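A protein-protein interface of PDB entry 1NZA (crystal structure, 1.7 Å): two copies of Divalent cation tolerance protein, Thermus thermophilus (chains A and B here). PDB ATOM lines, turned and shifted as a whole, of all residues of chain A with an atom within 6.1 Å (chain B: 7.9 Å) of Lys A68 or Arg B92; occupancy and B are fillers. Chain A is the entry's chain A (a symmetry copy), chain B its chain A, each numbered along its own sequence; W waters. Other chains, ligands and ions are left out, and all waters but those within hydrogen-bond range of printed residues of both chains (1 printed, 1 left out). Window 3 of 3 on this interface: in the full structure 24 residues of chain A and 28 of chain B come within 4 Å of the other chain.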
ATOM      1  N   ALA A  63      31.379  14.391 -11.975  1.00  0.00           N
ATOM      2  CA  ALA A  63      30.748  14.364 -10.663  1.00  0.00           C
ATOM      3  C   ALA A  63      29.322  13.837 -10.734  1.00  0.00           C
ATOM      4  O   ALA A  63      28.806  13.301  -9.756  1.00  0.00           O
ATOM      5  CB  ALA A  63      30.750  15.766 -10.052  1.00  0.00           C
ATOM      6  N   PHE A  64      28.696  13.969 -11.900  1.00  0.00           N
ATOM      7  CA  PHE A  64      27.311  13.541 -12.078  1.00  0.00           C
ATOM      8  C   PHE A  64      26.933  12.178 -11.502  1.00  0.00           C
ATOM      9  O   PHE A  64      25.925  12.061 -10.808  1.00  0.00           O
ATOM     10  CB  PHE A  64      26.915  13.582 -13.560  1.00  0.00           C
ATOM     11  CG  PHE A  64      25.434  13.465 -13.780  1.00  0.00           C
ATOM     12  CD1 PHE A  64      24.579  14.492 -13.389  1.00  0.00           C
ATOM     13  CD2 PHE A  64      24.889  12.317 -14.340  1.00  0.00           C
ATOM     14  CE1 PHE A  64      23.205  14.378 -13.544  1.00  0.00           C
ATOM     15  CE2 PHE A  64      23.509  12.189 -14.500  1.00  0.00           C
ATOM     16  CZ  PHE A  64      22.665  13.225 -14.102  1.00  0.00           C
ATOM     17  N   PRO A  65      27.716  11.122 -11.792  1.00  0.00           N
ATOM     18  CA  PRO A  65      27.373   9.804 -11.250  1.00  0.00           C
ATOM     19  C   PRO A  65      27.251   9.826  -9.727  1.00  0.00           C
ATOM     20  O   PRO A  65      26.339   9.225  -9.159  1.00  0.00           O
ATOM     21  CB  PRO A  65      28.530   8.922 -11.721  1.00  0.00           C
ATOM     22  CG  PRO A  65      28.944   9.572 -13.001  1.00  0.00           C
ATOM     23  CD  PRO A  65      28.907  11.041 -12.654  1.00  0.00           C
ATOM     24  N   LYS A  66      28.176  10.522  -9.075  1.00  0.00           N
ATOM     25  CA  LYS A  66      28.178  10.625  -7.622  1.00  0.00           C
ATOM     26  C   LYS A  66      27.041  11.534  -7.171  1.00  0.00           C
ATOM     27  O   LYS A  66      26.432  11.316  -6.125  1.00  0.00           O
ATOM     28  CB  LYS A  66      29.518  11.174  -7.123  1.00  0.00           C
ATOM     29  CG  LYS A  66      30.719  10.271  -7.394  1.00  0.00           C
ATOM     30  CD  LYS A  66      31.092  10.235  -8.870  1.00  0.00           C
ATOM     31  CE  LYS A  66      32.315   9.357  -9.106  1.00  0.00           C
ATOM     32  NZ  LYS A  66      32.706   9.306 -10.542  1.00  0.00           N
ATOM     33  N   LEU A  67      26.757  12.555  -7.970  1.00  0.00           N
ATOM     34  CA  LEU A  67      25.679  13.477  -7.651  1.00  0.00           C
ATOM     35  C   LEU A  67      24.351  12.731  -7.638  1.00  0.00           C
ATOM     36  O   LEU A  67      23.548  12.898  -6.719  1.00  0.00           O
ATOM     37  CB  LEU A  67      25.648  14.617  -8.671  1.00  0.00           C
ATOM     38  CG  LEU A  67      24.524  15.647  -8.564  1.00  0.00           C
ATOM     39  CD1 LEU A  67      24.958  16.938  -9.226  1.00  0.00           C
ATOM     40  CD2 LEU A  67      23.264  15.106  -9.208  1.00  0.00           C
ATOM     41  N   LYS A  68      24.113  11.902  -8.651  1.00  0.00           N
ATOM     42  CA  LYS A  68      22.869  11.142  -8.703  1.00  0.00           C
ATOM     43  C   LYS A  68      22.698  10.283  -7.457  1.00  0.00           C
ATOM     44  O   LYS A  68      21.614  10.231  -6.879  1.00  0.00           O
ATOM     45  CB  LYS A  68      22.817  10.232  -9.931  1.00  0.00           C
ATOM     46  CG  LYS A  68      22.492  10.940 -11.234  1.00  0.00           C
ATOM     47  CD  LYS A  68      22.092   9.936 -12.314  1.00  0.00           C
ATOM     48  CE  LYS A  68      23.195   8.914 -12.564  1.00  0.00           C
ATOM     49  NZ  LYS A  68      22.808   7.912 -13.598  1.00  0.00           N
ATOM     50  N   GLU A  69      23.767   9.598  -7.058  1.00  0.00           N
ATOM     51  CA  GLU A  69      23.724   8.741  -5.877  1.00  0.00           C
ATOM     52  C   GLU A  69      23.335   9.516  -4.629  1.00  0.00           C
ATOM     53  O   GLU A  69      22.457   9.098  -3.877  1.00  0.00           O
ATOM     54  CB  GLU A  69      25.080   8.067  -5.646  1.00  0.00           C
ATOM     55  CG  GLU A  69      25.311   6.832  -6.495  1.00  0.00           C
ATOM     56  CD  GLU A  69      26.640   6.162  -6.194  1.00  0.00           C
ATOM     57  OE1 GLU A  69      26.917   5.887  -5.005  1.00  0.00           O
ATOM     58  OE2 GLU A  69      27.405   5.904  -7.146  1.00  0.00           O
ATOM     59  N   ARG A  70      23.991  10.646  -4.408  1.00  0.00           N
ATOM     60  CA  ARG A  70      23.701  11.457  -3.236  1.00  0.00           C
ATOM     61  C   ARG A  70      22.281  12.016  -3.298  1.00  0.00           C
ATOM     62  O   ARG A  70      21.582  12.054  -2.288  1.00  0.00           O
ATOM     63  CB  ARG A  70      24.719  12.594  -3.114  1.00  0.00           C
ATOM     64  CG  ARG A  70      26.169  12.124  -3.047  1.00  0.00           C
ATOM     65  CD  ARG A  70      26.454  11.264  -1.812  1.00  0.00           C
ATOM     66  NE  ARG A  70      26.395  12.035  -0.571  1.00  0.00           N
ATOM     67  CZ  ARG A  70      25.518  11.822   0.405  1.00  0.00           C
ATOM     68  NH1 ARG A  70      24.613  10.855   0.290  1.00  0.00           N
ATOM     69  NH2 ARG A  70      25.546  12.573   1.499  1.00  0.00           N
ATOM     70  N   VAL A  71      21.845  12.441  -4.481  1.00  0.00           N
ATOM     71  CA  VAL A  71      20.501  12.991  -4.617  1.00  0.00           C
ATOM     72  C   VAL A  71      19.416  11.954  -4.340  1.00  0.00           C
ATOM     73  O   VAL A  71      18.443  12.240  -3.644  1.00  0.00           O
ATOM     74  CB  VAL A  71      20.278  13.589  -6.021  1.00  0.00           C
ATOM     75  CG1 VAL A  71      18.827  14.042  -6.167  1.00  0.00           C
ATOM     76  CG2 VAL A  71      21.218  14.759  -6.237  1.00  0.00           C
ATOM     77  N   LYS A  72      19.574  10.752  -4.884  1.00  0.00           N
ATOM     78  CA  LYS A  72      18.584   9.706  -4.659  1.00  0.00           C
ATOM     79  C   LYS A  72      18.484   9.377  -3.173  1.00  0.00           C
ATOM     80  O   LYS A  72      17.403   9.078  -2.667  1.00  0.00           O
ATOM     81  CB  LYS A  72      18.948   8.452  -5.455  1.00  0.00           C
ATOM     82  CG  LYS A  72      18.827   8.639  -6.957  1.00  0.00           C
ATOM     83  CD  LYS A  72      19.293   7.409  -7.710  1.00  0.00           C
ATOM     84  CE  LYS A  72      19.234   7.646  -9.209  1.00  0.00           C
ATOM     85  NZ  LYS A  72      19.811   6.508  -9.972  1.00  0.00           N
ATOM     86  N   ALA A  73      19.615   9.452  -2.475  1.00  0.00           N
ATOM     87  CA  ALA A  73      19.668   9.163  -1.045  1.00  0.00           C
ATOM     88  C   ALA A  73      18.947  10.223  -0.216  1.00  0.00           C
ATOM     89  O   ALA A  73      18.161   9.900   0.676  1.00  0.00           O
ATOM     90  CB  ALA A  73      21.119   9.053  -0.589  1.00  0.00           C
ATOM     91  N   ILE A  82      16.258  14.253 -12.201  1.00  0.00           N
ATOM     92  CA  ILE A  82      17.653  14.677 -12.233  1.00  0.00           C
ATOM     93  C   ILE A  82      18.045  14.677 -13.705  1.00  0.00           C
ATOM     94  O   ILE A  82      18.324  13.619 -14.272  1.00  0.00           O
ATOM     95  CB  ILE A  82      18.600  13.698 -11.501  1.00  0.00           C
ATOM     96  CG1 ILE A  82      18.054  13.370 -10.111  1.00  0.00           C
ATOM     97  CG2 ILE A  82      19.987  14.326 -11.374  1.00  0.00           C
ATOM     98  CD1 ILE A  82      18.917  12.388  -9.329  1.00  0.00           C
ATOM     99  N   GLU B   2      15.923  13.251 -25.368  1.00  0.00           N
ATOM    100  CA  GLU B   2      15.031  13.832 -24.368  1.00  0.00           C
ATOM    101  C   GLU B   2      15.386  15.310 -24.343  1.00  0.00           C
ATOM    102  O   GLU B   2      16.539  15.674 -24.565  1.00  0.00           O
ATOM    103  CB  GLU B   2      15.256  13.221 -22.984  1.00  0.00           C
ATOM    104  CG  GLU B   2      15.048  11.721 -22.907  1.00  0.00           C
ATOM    105  CD  GLU B   2      16.318  10.945 -23.190  1.00  0.00           C
ATOM    106  OE1 GLU B   2      16.334   9.719 -22.956  1.00  0.00           O
ATOM    107  OE2 GLU B   2      17.302  11.560 -23.648  1.00  0.00           O
ATOM    108  N   GLU B  89      22.265  13.937 -20.039  1.00  0.00           N
ATOM    109  CA  GLU B  89      22.166  12.756 -19.192  1.00  0.00           C
ATOM    110  C   GLU B  89      21.264  13.041 -17.999  1.00  0.00           C
ATOM    111  O   GLU B  89      20.811  14.169 -17.806  1.00  0.00           O
ATOM    112  CB  GLU B  89      23.552  12.331 -18.699  1.00  0.00           C
ATOM    113  CG  GLU B  89      24.363  13.437 -18.043  1.00  0.00           C
ATOM    114  CD  GLU B  89      25.701  12.943 -17.518  1.00  0.00           C
ATOM    115  OE1 GLU B  89      26.551  13.781 -17.152  1.00  0.00           O
ATOM    116  OE2 GLU B  89      25.900  11.711 -17.466  1.00  0.00           O
ATOM    117  N   GLY B  90      21.001  12.015 -17.201  1.00  0.00           N
ATOM    118  CA  GLY B  90      20.151  12.206 -16.044  1.00  0.00           C
ATOM    119  C   GLY B  90      19.829  10.910 -15.343  1.00  0.00           C
ATOM    120  O   GLY B  90      20.396   9.857 -15.650  1.00  0.00           O
ATOM    121  N   ASN B  91      18.919  10.990 -14.382  1.00  0.00           N
ATOM    122  CA  ASN B  91      18.501   9.807 -13.646  1.00  0.00           C
ATOM    123  C   ASN B  91      17.882   8.863 -14.671  1.00  0.00           C
ATOM    124  O   ASN B  91      16.818   9.146 -15.218  1.00  0.00           O
ATOM    125  CB  ASN B  91      17.476  10.204 -12.581  1.00  0.00           C
ATOM    126  CG  ASN B  91      16.970   9.021 -11.800  1.00  0.00           C
ATOM    127  OD1 ASN B  91      17.607   7.967 -11.777  1.00  0.00           O
ATOM    128  ND2 ASN B  91      15.825   9.185 -11.147  1.00  0.00           N
ATOM    129  N   ARG B  92      18.563   7.752 -14.942  1.00  0.00           N
ATOM    130  CA  ARG B  92      18.103   6.768 -15.924  1.00  0.00           C
ATOM    131  C   ARG B  92      16.640   6.366 -15.777  1.00  0.00           C
ATOM    132  O   ARG B  92      15.899   6.311 -16.763  1.00  0.00           O
ATOM    133  CB  ARG B  92      18.987   5.515 -15.862  1.00  0.00           C
ATOM    134  CG  ARG B  92      20.475   5.797 -16.043  1.00  0.00           C
ATOM    135  CD  ARG B  92      21.315   4.527 -15.923  1.00  0.00           C
ATOM    136  NE  ARG B  92      22.746   4.822 -15.864  1.00  0.00           N
ATOM    137  CZ  ARG B  92      23.427   5.431 -16.832  1.00  0.00           C
ATOM    138  NH1 ARG B  92      22.809   5.811 -17.941  1.00  0.00           N
ATOM    139  NH2 ARG B  92      24.725   5.669 -16.689  1.00  0.00           N
ATOM    140  N   GLU B  93      16.215   6.082 -14.551  1.00  0.00           N
ATOM    141  CA  GLU B  93      14.833   5.687 -14.320  1.00  0.00           C
ATOM    142  C   GLU B  93      13.875   6.846 -14.581  1.00  0.00           C
ATOM    143  O   GLU B  93      12.732   6.636 -14.989  1.00  0.00           O
ATOM    144  CB  GLU B  93      14.670   5.156 -12.895  1.00  0.00           C
ATOM    145  CG  GLU B  93      15.478   3.890 -12.645  1.00  0.00           C
ATOM    146  CD  GLU B  93      15.225   3.288 -11.279  1.00  0.00           C
ATOM    147  OE1 GLU B  93      14.065   2.915 -11.000  1.00  0.00           O
ATOM    148  OE2 GLU B  93      16.186   3.187 -10.487  1.00  0.00           O
ATOM    149  N   TYR B  94      14.343   8.071 -14.358  1.00  0.00           N
ATOM    150  CA  TYR B  94      13.503   9.238 -14.599  1.00  0.00           C
ATOM    151  C   TYR B  94      13.336   9.454 -16.098  1.00  0.00           C
ATOM    152  O   TYR B  94      12.236   9.726 -16.578  1.00  0.00           O
ATOM    153  CB  TYR B  94      14.113  10.498 -13.976  1.00  0.00           C
ATOM    154  CG  TYR B  94      13.261  11.727 -14.183  1.00  0.00           C
ATOM    155  CD1 TYR B  94      12.069  11.900 -13.479  1.00  0.00           C
ATOM    156  CD2 TYR B  94      13.617  12.697 -15.118  1.00  0.00           C
ATOM    157  CE1 TYR B  94      11.250  13.009 -13.702  1.00  0.00           C
ATOM    158  CE2 TYR B  94      12.806  13.806 -15.350  1.00  0.00           C
ATOM    159  CZ  TYR B  94      11.625  13.956 -14.637  1.00  0.00           C
ATOM    160  OH  TYR B  94      10.824  15.059 -14.851  1.00  0.00           O
ATOM    161  N   LEU B  95      14.431   9.328 -16.842  1.00  0.00           N
ATOM    162  CA  LEU B  95      14.376   9.518 -18.282  1.00  0.00           C
ATOM    163  C   LEU B  95      13.542   8.444 -18.974  1.00  0.00           C
ATOM    164  O   LEU B  95      12.903   8.712 -19.991  1.00  0.00           O
ATOM    165  CB  LEU B  95      15.789   9.550 -18.865  1.00  0.00           C
ATOM    166  CG  LEU B  95      16.639  10.750 -18.438  1.00  0.00           C
ATOM    167  CD1 LEU B  95      17.999  10.691 -19.124  1.00  0.00           C
ATOM    168  CD2 LEU B  95      15.916  12.042 -18.795  1.00  0.00           C
ATOM    169  N   ASP B  96      13.547   7.232 -18.428  1.00  0.00           N
ATOM    170  CA  ASP B  96      12.756   6.153 -19.011  1.00  0.00           C
ATOM    171  C   ASP B  96      11.286   6.502 -18.817  1.00  0.00           C
ATOM    172  O   ASP B  96      10.480   6.368 -19.738  1.00  0.00           O
ATOM    173  CB  ASP B  96      13.066   4.817 -18.331  1.00  0.00           C
ATOM    174  CG  ASP B  96      12.292   3.661 -18.945  1.00  0.00           C
ATOM    175  OD1 ASP B  96      12.378   3.483 -20.178  1.00  0.00           O
ATOM    176  OD2 ASP B  96      11.602   2.932 -18.197  1.00  0.00           O
ATOM    177  N   TRP B  97      10.948   6.952 -17.611  1.00  0.00           N
ATOM    178  CA  TRP B  97       9.582   7.350 -17.291  1.00  0.00           C
ATOM    179  C   TRP B  97       9.172   8.456 -18.252  1.00  0.00           C
ATOM    180  O   TRP B  97       8.031   8.514 -18.710  1.00  0.00           O
ATOM    181  CB  TRP B  97       9.509   7.872 -15.849  1.00  0.00           C
ATOM    182  CG  TRP B  97       8.229   8.603 -15.528  1.00  0.00           C
ATOM    183  CD1 TRP B  97       7.008   8.050 -15.250  1.00  0.00           C
ATOM    184  CD2 TRP B  97       8.041  10.025 -15.498  1.00  0.00           C
ATOM    185  NE1 TRP B  97       6.074   9.040 -15.052  1.00  0.00           N
ATOM    186  CE2 TRP B  97       6.680  10.261 -15.199  1.00  0.00           C
ATOM    187  CE3 TRP B  97       8.892  11.122 -15.696  1.00  0.00           C
ATOM    188  CZ2 TRP B  97       6.148  11.553 -15.093  1.00  0.00           C
ATOM    189  CZ3 TRP B  97       8.364  12.408 -15.590  1.00  0.00           C
ATOM    190  CH2 TRP B  97       7.001  12.609 -15.291  1.00  0.00           C
ATOM    191  N   LEU B  98      10.123   9.334 -18.555  1.00  0.00           N
ATOM    192  CA  LEU B  98       9.886  10.455 -19.453  1.00  0.00           C
ATOM    193  C   LEU B  98       9.524   9.962 -20.853  1.00  0.00           C
ATOM    194  O   LEU B  98       8.549  10.421 -21.445  1.00  0.00           O
ATOM    195  CB  LEU B  98      11.132  11.349 -19.498  1.00  0.00           C
ATOM    196  CG  LEU B  98      11.056  12.712 -20.190  1.00  0.00           C
ATOM    197  CD1 LEU B  98      12.313  13.508 -19.868  1.00  0.00           C
ATOM    198  CD2 LEU B  98      10.906  12.542 -21.697  1.00  0.00           C
ATOM    199  N   ARG B  99      10.306   9.026 -21.384  1.00  0.00           N
ATOM    200  CA  ARG B  99      10.032   8.493 -22.713  1.00  0.00           C
ATOM    201  C   ARG B  99       8.761   7.649 -22.691  1.00  0.00           C
ATOM    202  O   ARG B  99       7.897   7.782 -23.555  1.00  0.00           O
ATOM    203  CB  ARG B  99      11.214   7.653 -23.203  1.00  0.00           C
ATOM    204  CG  ARG B  99      12.495   8.448 -23.389  1.00  0.00           C
ATOM    205  CD  ARG B  99      13.550   7.612 -24.093  1.00  0.00           C
ATOM    206  NE  ARG B  99      13.898   6.409 -23.344  1.00  0.00           N
ATOM    207  CZ  ARG B  99      14.752   6.377 -22.325  1.00  0.00           C
ATOM    208  NH1 ARG B  99      15.358   7.486 -21.927  1.00  0.00           N
ATOM    209  NH2 ARG B  99      14.997   5.233 -21.700  1.00  0.00           N
HETATM  210  O   HOH W   1      25.846   7.657 -14.258  1.00  0.00           O
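The backbone NH (N) of Asn B91 lies within hydrogen-bond range of the backbone carbonyl oxygen (O) of Ile A82, 2.7 Å away. NZ of Lys A72 lies close to OD1 of Asn B91, at 3.2 Å.
Among the printed residues, merely in contact across the chains: Phe A64 with Glu B89, Phe A64 with Gly B90, Lys A68 with Gly B90, Lys A68 with Asn B91, Lys A68 with Arg B92 and Ile A82 with Gly B90.
Water W1 lies within hydrogen-bond range of the side-chain amino group (NZ) of Lys A68 (3.1 Å) and the guanidinium group (NH2) of Arg B92 (3.3 Å).
Of the 12 printed residues of chain A, 4 touch a printed residue of chain B. Of the 12 printed residues of chain B, 4 touch a printed residue of chain A. Along chain B the printed residues that touch a printed residue of chain A span positions 89 to 92. Among the printed residues, no Asp or Glu carboxylate lies within 4 Å of a Lys or Arg side-chain nitrogen of the other chain.
Arg B92 touches one residue of chain A. Printed residues of chain A within 4 Å of Gly B90: Phe A64, Lys A68 and Ile A82. Of the printed residues of chain A, Glu B89 touches Phe A64. Of the printed residues of chain A, Asn B91 touches Lys A68, Lys A72 and Ile A82. The nearest residue of chain B that does not touch Lys A68 is Glu B89 (6.2 Å).
No position is printed for both chains. Of the 8 pairs that touch across the chains among the printed residues, none has its exchanged pair printed and touching as well.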
